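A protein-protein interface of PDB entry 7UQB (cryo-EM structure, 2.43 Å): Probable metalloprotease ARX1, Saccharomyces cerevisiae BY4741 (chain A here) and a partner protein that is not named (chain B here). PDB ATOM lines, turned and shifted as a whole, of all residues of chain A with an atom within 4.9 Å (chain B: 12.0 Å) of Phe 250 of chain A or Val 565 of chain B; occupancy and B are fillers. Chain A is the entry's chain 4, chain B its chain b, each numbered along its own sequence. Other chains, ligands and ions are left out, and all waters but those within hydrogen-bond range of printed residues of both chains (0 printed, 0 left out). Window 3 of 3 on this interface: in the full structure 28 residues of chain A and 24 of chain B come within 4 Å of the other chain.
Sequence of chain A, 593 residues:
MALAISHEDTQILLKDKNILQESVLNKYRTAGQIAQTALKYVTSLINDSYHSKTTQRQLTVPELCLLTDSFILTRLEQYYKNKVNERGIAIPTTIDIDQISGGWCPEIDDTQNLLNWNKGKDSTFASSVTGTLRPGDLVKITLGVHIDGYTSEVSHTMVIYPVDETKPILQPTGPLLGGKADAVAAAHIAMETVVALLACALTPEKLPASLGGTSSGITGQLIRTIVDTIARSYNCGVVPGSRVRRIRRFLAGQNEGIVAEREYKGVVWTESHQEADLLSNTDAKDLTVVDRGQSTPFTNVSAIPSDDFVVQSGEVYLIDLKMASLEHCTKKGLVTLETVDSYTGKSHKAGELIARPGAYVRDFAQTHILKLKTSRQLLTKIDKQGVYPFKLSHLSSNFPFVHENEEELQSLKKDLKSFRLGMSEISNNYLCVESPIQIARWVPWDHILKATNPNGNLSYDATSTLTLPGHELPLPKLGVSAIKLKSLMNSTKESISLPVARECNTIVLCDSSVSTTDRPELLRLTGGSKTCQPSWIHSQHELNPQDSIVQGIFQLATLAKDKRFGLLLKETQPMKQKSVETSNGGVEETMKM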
ATOM      1  N   GLU A  86     -26.651 -29.784  -9.492  1.00  0.00           N
ATOM      2  CA  GLU A  86     -26.930 -28.355  -9.582  1.00  0.00           C
ATOM      3  C   GLU A  86     -26.332 -27.787 -10.861  1.00  0.00           C
ATOM      4  O   GLU A  86     -25.127 -27.917 -11.098  1.00  0.00           O
ATOM      5  CB  GLU A  86     -26.369 -27.614  -8.366  1.00  0.00           C
ATOM      6  CG  GLU A  86     -26.701 -28.268  -7.035  1.00  0.00           C
ATOM      7  CD  GLU A  86     -26.066 -27.559  -5.858  1.00  0.00           C
ATOM      8  OE1 GLU A  86     -25.556 -26.434  -6.043  1.00  0.00           O
ATOM      9  OE2 GLU A  86     -26.074 -28.129  -4.746  1.00  0.00           O
ATOM     10  N   ASP A 148     -22.432 -27.948 -12.146  1.00  0.00           N
ATOM     11  CA  ASP A 148     -21.873 -28.609 -10.962  1.00  0.00           C
ATOM     12  C   ASP A 148     -20.983 -27.663 -10.156  1.00  0.00           C
ATOM     13  O   ASP A 148     -20.032 -28.091  -9.500  1.00  0.00           O
ATOM     14  CB  ASP A 148     -21.104 -29.881 -11.343  1.00  0.00           C
ATOM     15  CG  ASP A 148     -20.991 -30.864 -10.193  1.00  0.00           C
ATOM     16  OD1 ASP A 148     -21.646 -30.644  -9.154  1.00  0.00           O
ATOM     17  OD2 ASP A 148     -20.241 -31.854 -10.327  1.00  0.00           O
ATOM     18  N   GLY A 149     -21.284 -26.368 -10.201  1.00  0.00           N
ATOM     19  CA  GLY A 149     -20.487 -25.372  -9.519  1.00  0.00           C
ATOM     20  C   GLY A 149     -19.256 -24.908 -10.263  1.00  0.00           C
ATOM     21  O   GLY A 149     -18.560 -24.012  -9.770  1.00  0.00           O
ATOM     22  N   ARG A 248     -12.393 -21.809  -8.006  1.00  0.00           N
ATOM     23  CA  ARG A 248     -12.615 -23.202  -7.639  1.00  0.00           C
ATOM     24  C   ARG A 248     -14.099 -23.531  -7.791  1.00  0.00           C
ATOM     25  O   ARG A 248     -14.890 -22.718  -8.276  1.00  0.00           O
ATOM     26  CB  ARG A 248     -12.122 -23.480  -6.215  1.00  0.00           C
ATOM     27  CG  ARG A 248     -10.616 -23.333  -6.058  1.00  0.00           C
ATOM     28  CD  ARG A 248     -10.076 -24.082  -4.847  1.00  0.00           C
ATOM     29  NE  ARG A 248     -10.329 -23.383  -3.593  1.00  0.00           N
ATOM     30  CZ  ARG A 248     -11.031 -23.879  -2.584  1.00  0.00           C
ATOM     31  NH1 ARG A 248     -11.553 -25.093  -2.636  1.00  0.00           N
ATOM     32  NH2 ARG A 248     -11.207 -23.142  -1.491  1.00  0.00           N
ATOM     33  N   ARG A 249     -14.477 -24.740  -7.382  1.00  0.00           N
ATOM     34  CA  ARG A 249     -15.871 -25.155  -7.474  1.00  0.00           C
ATOM     35  C   ARG A 249     -16.706 -24.410  -6.440  1.00  0.00           C
ATOM     36  O   ARG A 249     -16.363 -24.384  -5.254  1.00  0.00           O
ATOM     37  CB  ARG A 249     -15.996 -26.664  -7.274  1.00  0.00           C
ATOM     38  CG  ARG A 249     -17.422 -27.193  -7.374  1.00  0.00           C
ATOM     39  CD  ARG A 249     -17.441 -28.712  -7.460  1.00  0.00           C
ATOM     40  NE  ARG A 249     -18.787 -29.249  -7.623  1.00  0.00           N
ATOM     41  CZ  ARG A 249     -19.442 -29.930  -6.693  1.00  0.00           C
ATOM     42  NH1 ARG A 249     -18.900 -30.188  -5.514  1.00  0.00           N
ATOM     43  NH2 ARG A 249     -20.671 -30.366  -6.954  1.00  0.00           N
ATOM     44  N   PHE A 250     -17.786 -23.777  -6.906  1.00  0.00           N
ATOM     45  CA  PHE A 250     -18.731 -22.958  -6.147  1.00  0.00           C
ATOM     46  C   PHE A 250     -18.117 -21.668  -5.619  1.00  0.00           C
ATOM     47  O   PHE A 250     -18.835 -20.863  -5.017  1.00  0.00           O
ATOM     48  CB  PHE A 250     -19.369 -23.711  -4.968  1.00  0.00           C
ATOM     49  CG  PHE A 250     -20.332 -24.780  -5.381  1.00  0.00           C
ATOM     50  CD1 PHE A 250     -21.491 -24.455  -6.063  1.00  0.00           C
ATOM     51  CD2 PHE A 250     -20.090 -26.107  -5.070  1.00  0.00           C
ATOM     52  CE1 PHE A 250     -22.385 -25.436  -6.440  1.00  0.00           C
ATOM     53  CE2 PHE A 250     -20.982 -27.090  -5.444  1.00  0.00           C
ATOM     54  CZ  PHE A 250     -22.129 -26.753  -6.131  1.00  0.00           C
ATOM     55  N   LEU A 251     -16.823 -21.436  -5.827  1.00  0.00           N
ATOM     56  CA  LEU A 251     -16.124 -20.257  -5.328  1.00  0.00           C
ATOM     57  C   LEU A 251     -15.548 -19.532  -6.537  1.00  0.00           C
ATOM     58  O   LEU A 251     -14.377 -19.702  -6.881  1.00  0.00           O
ATOM     59  CB  LEU A 251     -15.039 -20.654  -4.334  1.00  0.00           C
ATOM     60  CG  LEU A 251     -15.517 -21.453  -3.121  1.00  0.00           C
ATOM     61  CD1 LEU A 251     -14.383 -22.279  -2.551  1.00  0.00           C
ATOM     62  CD2 LEU A 251     -16.087 -20.526  -2.064  1.00  0.00           C
ATOM     63  N   ALA A 252     -16.375 -18.706  -7.173  1.00  0.00           N
ATOM     64  CA  ALA A 252     -15.979 -17.980  -8.370  1.00  0.00           C
ATOM     65  C   ALA A 252     -16.037 -16.472  -8.183  1.00  0.00           C
ATOM     66  O   ALA A 252     -15.905 -15.732  -9.164  1.00  0.00           O
ATOM     67  CB  ALA A 252     -16.854 -18.389  -9.558  1.00  0.00           C
ATOM     68  N   GLN A 254     -18.768 -14.943  -7.400  1.00  0.00           N
ATOM     69  CA  GLN A 254     -20.049 -14.534  -7.967  1.00  0.00           C
ATOM     70  C   GLN A 254     -20.706 -13.446  -7.130  1.00  0.00           C
ATOM     71  O   GLN A 254     -21.474 -12.637  -7.659  1.00  0.00           O
ATOM     72  CB  GLN A 254     -20.977 -15.742  -8.111  1.00  0.00           C
ATOM     73  CG  GLN A 254     -21.211 -16.530  -6.829  1.00  0.00           C
ATOM     74  CD  GLN A 254     -20.317 -17.749  -6.708  1.00  0.00           C
ATOM     75  OE1 GLN A 254     -19.193 -17.762  -7.208  1.00  0.00           O
ATOM     76  NE2 GLN A 254     -20.818 -18.786  -6.047  1.00  0.00           N
ATOM     77  N   VAL A 387     -26.038 -21.152  -4.717  1.00  0.00           N
ATOM     78  CA  VAL A 387     -25.252 -20.102  -4.079  1.00  0.00           C
ATOM     79  C   VAL A 387     -24.886 -19.016  -5.081  1.00  0.00           C
ATOM     80  O   VAL A 387     -23.860 -18.343  -4.934  1.00  0.00           O
ATOM     81  CB  VAL A 387     -23.990 -20.689  -3.426  1.00  0.00           C
ATOM     82  CG1 VAL A 387     -24.362 -21.492  -2.198  1.00  0.00           C
ATOM     83  CG2 VAL A 387     -23.233 -21.556  -4.423  1.00  0.00           C
ATOM     84  N   TYR A 388     -25.713 -18.832  -6.098  1.00  0.00           N
ATOM     85  CA  TYR A 388     -25.435 -17.805  -7.085  1.00  0.00           C
ATOM     86  C   TYR A 388     -26.499 -16.713  -7.041  1.00  0.00           C
ATOM     87  O   TYR A 388     -27.636 -16.967  -6.633  1.00  0.00           O
ATOM     88  CB  TYR A 388     -25.370 -18.410  -8.492  1.00  0.00           C
ATOM     89  CG  TYR A 388     -24.190 -19.330  -8.678  1.00  0.00           C
ATOM     90  CD1 TYR A 388     -22.960 -18.835  -9.086  1.00  0.00           C
ATOM     91  CD2 TYR A 388     -24.299 -20.690  -8.429  1.00  0.00           C
ATOM     92  CE1 TYR A 388     -21.877 -19.668  -9.254  1.00  0.00           C
ATOM     93  CE2 TYR A 388     -23.219 -21.533  -8.593  1.00  0.00           C
ATOM     94  CZ  TYR A 388     -22.011 -21.016  -9.004  1.00  0.00           C
ATOM     95  OH  TYR A 388     -20.930 -21.851  -9.170  1.00  0.00           O
ATOM     96  N   TYR B 558     -25.974 -38.336   2.751  1.00  0.00           N
ATOM     97  CA  TYR B 558     -25.736 -36.901   2.756  1.00  0.00           C
ATOM     98  C   TYR B 558     -24.698 -36.583   1.689  1.00  0.00           C
ATOM     99  O   TYR B 558     -23.591 -37.132   1.711  1.00  0.00           O
ATOM    100  CB  TYR B 558     -25.259 -36.426   4.129  1.00  0.00           C
ATOM    101  CG  TYR B 558     -24.496 -35.120   4.090  1.00  0.00           C
ATOM    102  CD1 TYR B 558     -25.159 -33.910   3.934  1.00  0.00           C
ATOM    103  CD2 TYR B 558     -23.111 -35.097   4.213  1.00  0.00           C
ATOM    104  CE1 TYR B 558     -24.465 -32.715   3.895  1.00  0.00           C
ATOM    105  CE2 TYR B 558     -22.409 -33.907   4.174  1.00  0.00           C
ATOM    106  CZ  TYR B 558     -23.092 -32.719   4.017  1.00  0.00           C
ATOM    107  OH  TYR B 558     -22.397 -31.532   3.981  1.00  0.00           O
ATOM    108  N   VAL B 559     -25.056 -35.701   0.761  1.00  0.00           N
ATOM    109  CA  VAL B 559     -24.153 -35.242  -0.286  1.00  0.00           C
ATOM    110  C   VAL B 559     -23.945 -33.747  -0.100  1.00  0.00           C
ATOM    111  O   VAL B 559     -24.914 -33.001   0.083  1.00  0.00           O
ATOM    112  CB  VAL B 559     -24.696 -35.555  -1.693  1.00  0.00           C
ATOM    113  CG1 VAL B 559     -23.695 -35.122  -2.756  1.00  0.00           C
ATOM    114  CG2 VAL B 559     -25.004 -37.035  -1.825  1.00  0.00           C
ATOM    115  N   GLU B 560     -22.683 -33.321  -0.121  1.00  0.00           N
ATOM    116  CA  GLU B 560     -22.356 -31.912   0.045  1.00  0.00           C
ATOM    117  C   GLU B 560     -22.942 -31.087  -1.094  1.00  0.00           C
ATOM    118  O   GLU B 560     -22.784 -31.426  -2.271  1.00  0.00           O
ATOM    119  CB  GLU B 560     -20.840 -31.736   0.105  1.00  0.00           C
ATOM    120  CG  GLU B 560     -20.181 -32.455   1.270  1.00  0.00           C
ATOM    121  CD  GLU B 560     -18.738 -32.826   0.989  1.00  0.00           C
ATOM    122  OE1 GLU B 560     -18.406 -33.083  -0.187  1.00  0.00           O
ATOM    123  OE2 GLU B 560     -17.933 -32.860   1.944  1.00  0.00           O
ATOM    124  N   ARG B 561     -23.619 -30.001  -0.742  1.00  0.00           N
ATOM    125  CA  ARG B 561     -24.224 -29.096  -1.705  1.00  0.00           C
ATOM    126  C   ARG B 561     -23.442 -27.785  -1.739  1.00  0.00           C
ATOM    127  O   ARG B 561     -22.499 -27.571  -0.968  1.00  0.00           O
ATOM    128  CB  ARG B 561     -25.702 -28.865  -1.372  1.00  0.00           C
ATOM    129  CG  ARG B 561     -26.546 -30.137  -1.379  1.00  0.00           C
ATOM    130  CD  ARG B 561     -28.027 -29.847  -1.598  1.00  0.00           C
ATOM    131  NE  ARG B 561     -28.676 -29.263  -0.431  1.00  0.00           N
ATOM    132  CZ  ARG B 561     -29.456 -29.931   0.409  1.00  0.00           C
ATOM    133  NH1 ARG B 561     -29.703 -31.221   0.247  1.00  0.00           N
ATOM    134  NH2 ARG B 561     -30.007 -29.288   1.434  1.00  0.00           N
ATOM    135  N   GLY B 562     -23.837 -26.905  -2.662  1.00  0.00           N
ATOM    136  CA  GLY B 562     -23.157 -25.626  -2.795  1.00  0.00           C
ATOM    137  C   GLY B 562     -23.278 -24.766  -1.552  1.00  0.00           C
ATOM    138  O   GLY B 562     -22.357 -24.018  -1.209  1.00  0.00           O
ATOM    139  N   SER B 563     -24.420 -24.853  -0.864  1.00  0.00           N
ATOM    140  CA  SER B 563     -24.582 -24.139   0.396  1.00  0.00           C
ATOM    141  C   SER B 563     -23.612 -24.659   1.449  1.00  0.00           C
ATOM    142  O   SER B 563     -23.061 -23.877   2.231  1.00  0.00           O
ATOM    143  CB  SER B 563     -26.026 -24.254   0.882  1.00  0.00           C
ATOM    144  OG  SER B 563     -26.452 -25.604   0.913  1.00  0.00           O
ATOM    145  N   ASP B 564     -23.382 -25.974   1.476  1.00  0.00           N
ATOM    146  CA  ASP B 564     -22.368 -26.531   2.366  1.00  0.00           C
ATOM    147  C   ASP B 564     -20.976 -26.044   1.985  1.00  0.00           C
ATOM    148  O   ASP B 564     -20.142 -25.783   2.859  1.00  0.00           O
ATOM    149  CB  ASP B 564     -22.414 -28.058   2.334  1.00  0.00           C
ATOM    150  CG  ASP B 564     -23.817 -28.603   2.477  1.00  0.00           C
ATOM    151  OD1 ASP B 564     -24.647 -27.946   3.139  1.00  0.00           O
ATOM    152  OD2 ASP B 564     -24.089 -29.688   1.924  1.00  0.00           O
ATOM    153  N   VAL B 565     -20.704 -25.935   0.683  1.00  0.00           N
ATOM    154  CA  VAL B 565     -19.374 -25.535   0.230  1.00  0.00           C
ATOM    155  C   VAL B 565     -19.090 -24.080   0.592  1.00  0.00           C
ATOM    156  O   VAL B 565     -17.993 -23.746   1.054  1.00  0.00           O
ATOM    157  CB  VAL B 565     -19.233 -25.786  -1.284  1.00  0.00           C
ATOM    158  CG1 VAL B 565     -17.927 -25.211  -1.805  1.00  0.00           C
ATOM    159  CG2 VAL B 565     -19.309 -27.276  -1.577  1.00  0.00           C
ATOM    160  N   VAL B 566     -20.068 -23.197   0.403  1.00  0.00           N
ATOM    161  CA  VAL B 566     -19.828 -21.765   0.561  1.00  0.00           C
ATOM    162  C   VAL B 566     -20.116 -21.305   1.987  1.00  0.00           C
ATOM    163  O   VAL B 566     -19.261 -20.689   2.633  1.00  0.00           O
ATOM    164  CB  VAL B 566     -20.660 -20.954  -0.448  1.00  0.00           C
ATOM    165  CG1 VAL B 566     -20.375 -19.468  -0.295  1.00  0.00           C
ATOM    166  CG2 VAL B 566     -20.364 -21.410  -1.866  1.00  0.00           C
ATOM    167  N   PHE B 567     -21.317 -21.594   2.487  1.00  0.00           N
ATOM    168  CA  PHE B 567     -21.789 -21.070   3.760  1.00  0.00           C
ATOM    169  C   PHE B 567     -21.644 -22.060   4.908  1.00  0.00           C
ATOM    170  O   PHE B 567     -22.206 -21.827   5.982  1.00  0.00           O
ATOM    171  CB  PHE B 567     -23.256 -20.644   3.642  1.00  0.00           C
ATOM    172  CG  PHE B 567     -23.482 -19.501   2.696  1.00  0.00           C
ATOM    173  CD1 PHE B 567     -23.692 -19.730   1.347  1.00  0.00           C
ATOM    174  CD2 PHE B 567     -23.499 -18.197   3.160  1.00  0.00           C
ATOM    175  CE1 PHE B 567     -23.904 -18.681   0.478  1.00  0.00           C
ATOM    176  CE2 PHE B 567     -23.712 -17.144   2.296  1.00  0.00           C
ATOM    177  CZ  PHE B 567     -23.915 -17.385   0.954  1.00  0.00           C
ATOM    178  N   GLY B 568     -20.919 -23.161   4.705  1.00  0.00           N
ATOM    179  CA  GLY B 568     -20.838 -24.181   5.738  1.00  0.00           C
ATOM    180  C   GLY B 568     -20.115 -23.715   6.988  1.00  0.00           C
ATOM    181  O   GLY B 568     -20.570 -23.964   8.108  1.00  0.00           O
ATOM    182  N   ASP B 569     -18.987 -23.029   6.819  1.00  0.00           N
ATOM    183  CA  ASP B 569     -18.172 -22.584   7.941  1.00  0.00           C
ATOM    184  C   ASP B 569     -18.327 -21.101   8.251  1.00  0.00           C
ATOM    185  O   ASP B 569     -17.601 -20.583   9.105  1.00  0.00           O
ATOM    186  CB  ASP B 569     -16.696 -22.903   7.677  1.00  0.00           C
ATOM    187  CG  ASP B 569     -16.231 -22.423   6.317  1.00  0.00           C
ATOM    188  OD1 ASP B 569     -17.053 -21.855   5.566  1.00  0.00           O
ATOM    189  OD2 ASP B 569     -15.042 -22.620   5.996  1.00  0.00           O
ATOM    190  N   GLN B 570     -19.241 -20.406   7.584  1.00  0.00           N
ATOM    191  CA  GLN B 570     -19.421 -18.979   7.780  1.00  0.00           C
ATOM    192  C   GLN B 570     -20.706 -18.710   8.557  1.00  0.00           C
ATOM    193  O   GLN B 570     -21.440 -19.625   8.938  1.00  0.00           O
ATOM    194  CB  GLN B 570     -19.430 -18.253   6.433  1.00  0.00           C
ATOM    195  CG  GLN B 570     -18.113 -18.339   5.688  1.00  0.00           C
ATOM    196  CD  GLN B 570     -18.149 -17.620   4.357  1.00  0.00           C
ATOM    197  OE1 GLN B 570     -19.207 -17.191   3.898  1.00  0.00           O
ATOM    198  NE2 GLN B 570     -16.987 -17.484   3.730  1.00  0.00           N
ATOM    199  N   ASP B 571     -20.977 -17.433   8.793  1.00  0.00           N
ATOM    200  CA  ASP B 571     -22.180 -17.016   9.499  1.00  0.00           C
ATOM    201  C   ASP B 571     -22.495 -15.581   9.096  1.00  0.00           C
ATOM    202  O   ASP B 571     -21.886 -15.033   8.170  1.00  0.00           O
ATOM    203  CB  ASP B 571     -22.001 -17.159  11.014  1.00  0.00           C
ATOM    204  CG  ASP B 571     -23.285 -17.548  11.718  1.00  0.00           C
ATOM    205  OD1 ASP B 571     -24.182 -18.107  11.051  1.00  0.00           O
ATOM    206  OD2 ASP B 571     -23.400 -17.293  12.934  1.00  0.00           O
ATOM    207  N   LEU B 573     -23.123 -12.540   7.610  1.00  0.00           N
ATOM    208  CA  LEU B 573     -23.216 -11.852   6.321  1.00  0.00           C
ATOM    209  C   LEU B 573     -23.929 -10.512   6.427  1.00  0.00           C
ATOM    210  O   LEU B 573     -24.004  -9.784   5.433  1.00  0.00           O
ATOM    211  CB  LEU B 573     -23.908 -12.691   5.236  1.00  0.00           C
ATOM    212  CG  LEU B 573     -23.251 -12.671   3.859  1.00  0.00           C
ATOM    213  CD1 LEU B 573     -21.935 -13.428   3.917  1.00  0.00           C
ATOM    214  CD2 LEU B 573     -24.174 -13.255   2.804  1.00  0.00           C
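The backbone NH (N) of Gly 562 of chain B sits at hydrogen-bond distance from the side-chain carboxylate (OE2) of Glu 86 of chain A.
Of chain B, only Gly 562, Val 565 and Val 566 come within 4 Å of Phe 250 of chain A. Val 565 of chain B touches just these residues of chain A: Arg 249 (3.9 Å) and Phe 250 (3.8 Å). Glu 86 of chain A touches just these residues of chain B: Arg 561 (3.5 Å) and Gly 562 (3.3 Å). No residue of chain B comes within 4 Å of Asp 148 of chain A. No residue of chain B comes within 4 Å of Gly 149 of chain A. Of chain B, only Val 565 comes within 4 Å of Arg 249 of chain A. Val 387 of chain A touches just these residues of chain B: Gly 562 (3.4 Å), Ser 563 (3.6 Å), Val 566 (3.8 Å) and Phe 567 (3.9 Å). Of the printed residues of chain A, Gly 562 of chain B touches Glu 86 (3.3 Å), Phe 250 (3.7 Å) and Val 387 (3.4 Å). Of the printed residues of chain A, Ser 563 of chain B touches Val 387. Asp 564 of chain B touches none of the printed residues of chain A. The nearest printed residue of chain A that does not touch Gly 562 of chain B is Arg 249 of chain A (6.4 Å).
Glu 86 of chain A touches Arg 561 of chain B (OE2 to CB, 3.5 Å). CG1 of Val 565 of chain B touches O of Arg 249 of chain A, 3.9 Å away. Gly 562 of chain B touches Phe 250 of chain A (CA to CZ, 3.7 Å). Val 565 of chain B touches Phe 250 of chain A (CG2 to CD2, 3.8 Å). Phe 250 of chain A touches Val 566 of chain B. Val 387 of chain A touches Gly 562 of chain B. N of Ser 563 of chain B touches CG1 of Val 387 of chain A, 3.6 Å away. Val 566 of chain B touches Val 387 of chain A (CG2 to CG2, 3.8 Å). CG1 of Val 387 of chain A touches CE1 of Phe 567 of chain B (3.9 Å).
Of the 11 printed residues of chain A, 4 touch a printed residue of chain B. Printed residues of chain A that touch a printed residue of chain B: Glu 86, Arg 249, Phe 250 and Val 387. Hydrophobic or aromatic side chains of chain A that line the printed part of chain B: Phe 250 and Val 387.
OD2 of Asp 564 of chain B lies within hydrogen-bond range of N of Arg 561 of chain B (2.7 Å). O of Glu 86 of chain A lies within hydrogen-bond range of N of Asp 148 of chain A (2.9 Å). NH2 of Arg 249 of chain A lies within salt-bridge range of OD1 of Asp 148 of chain A (2.4 Å). The backbone carbonyl oxygen of Gly 149 of chain A lies within hydrogen-bond range of the backbone NH of Phe 250 of chain A, at 3.0 Å. O of Phe 250 of chain A lies within hydrogen-bond range of NE2 of Gln 254 of chain A, at 3.1 Å. O of Val 387 of chain A lies within hydrogen-bond range of NE2 of Gln 254 of chain A (3.3 Å).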
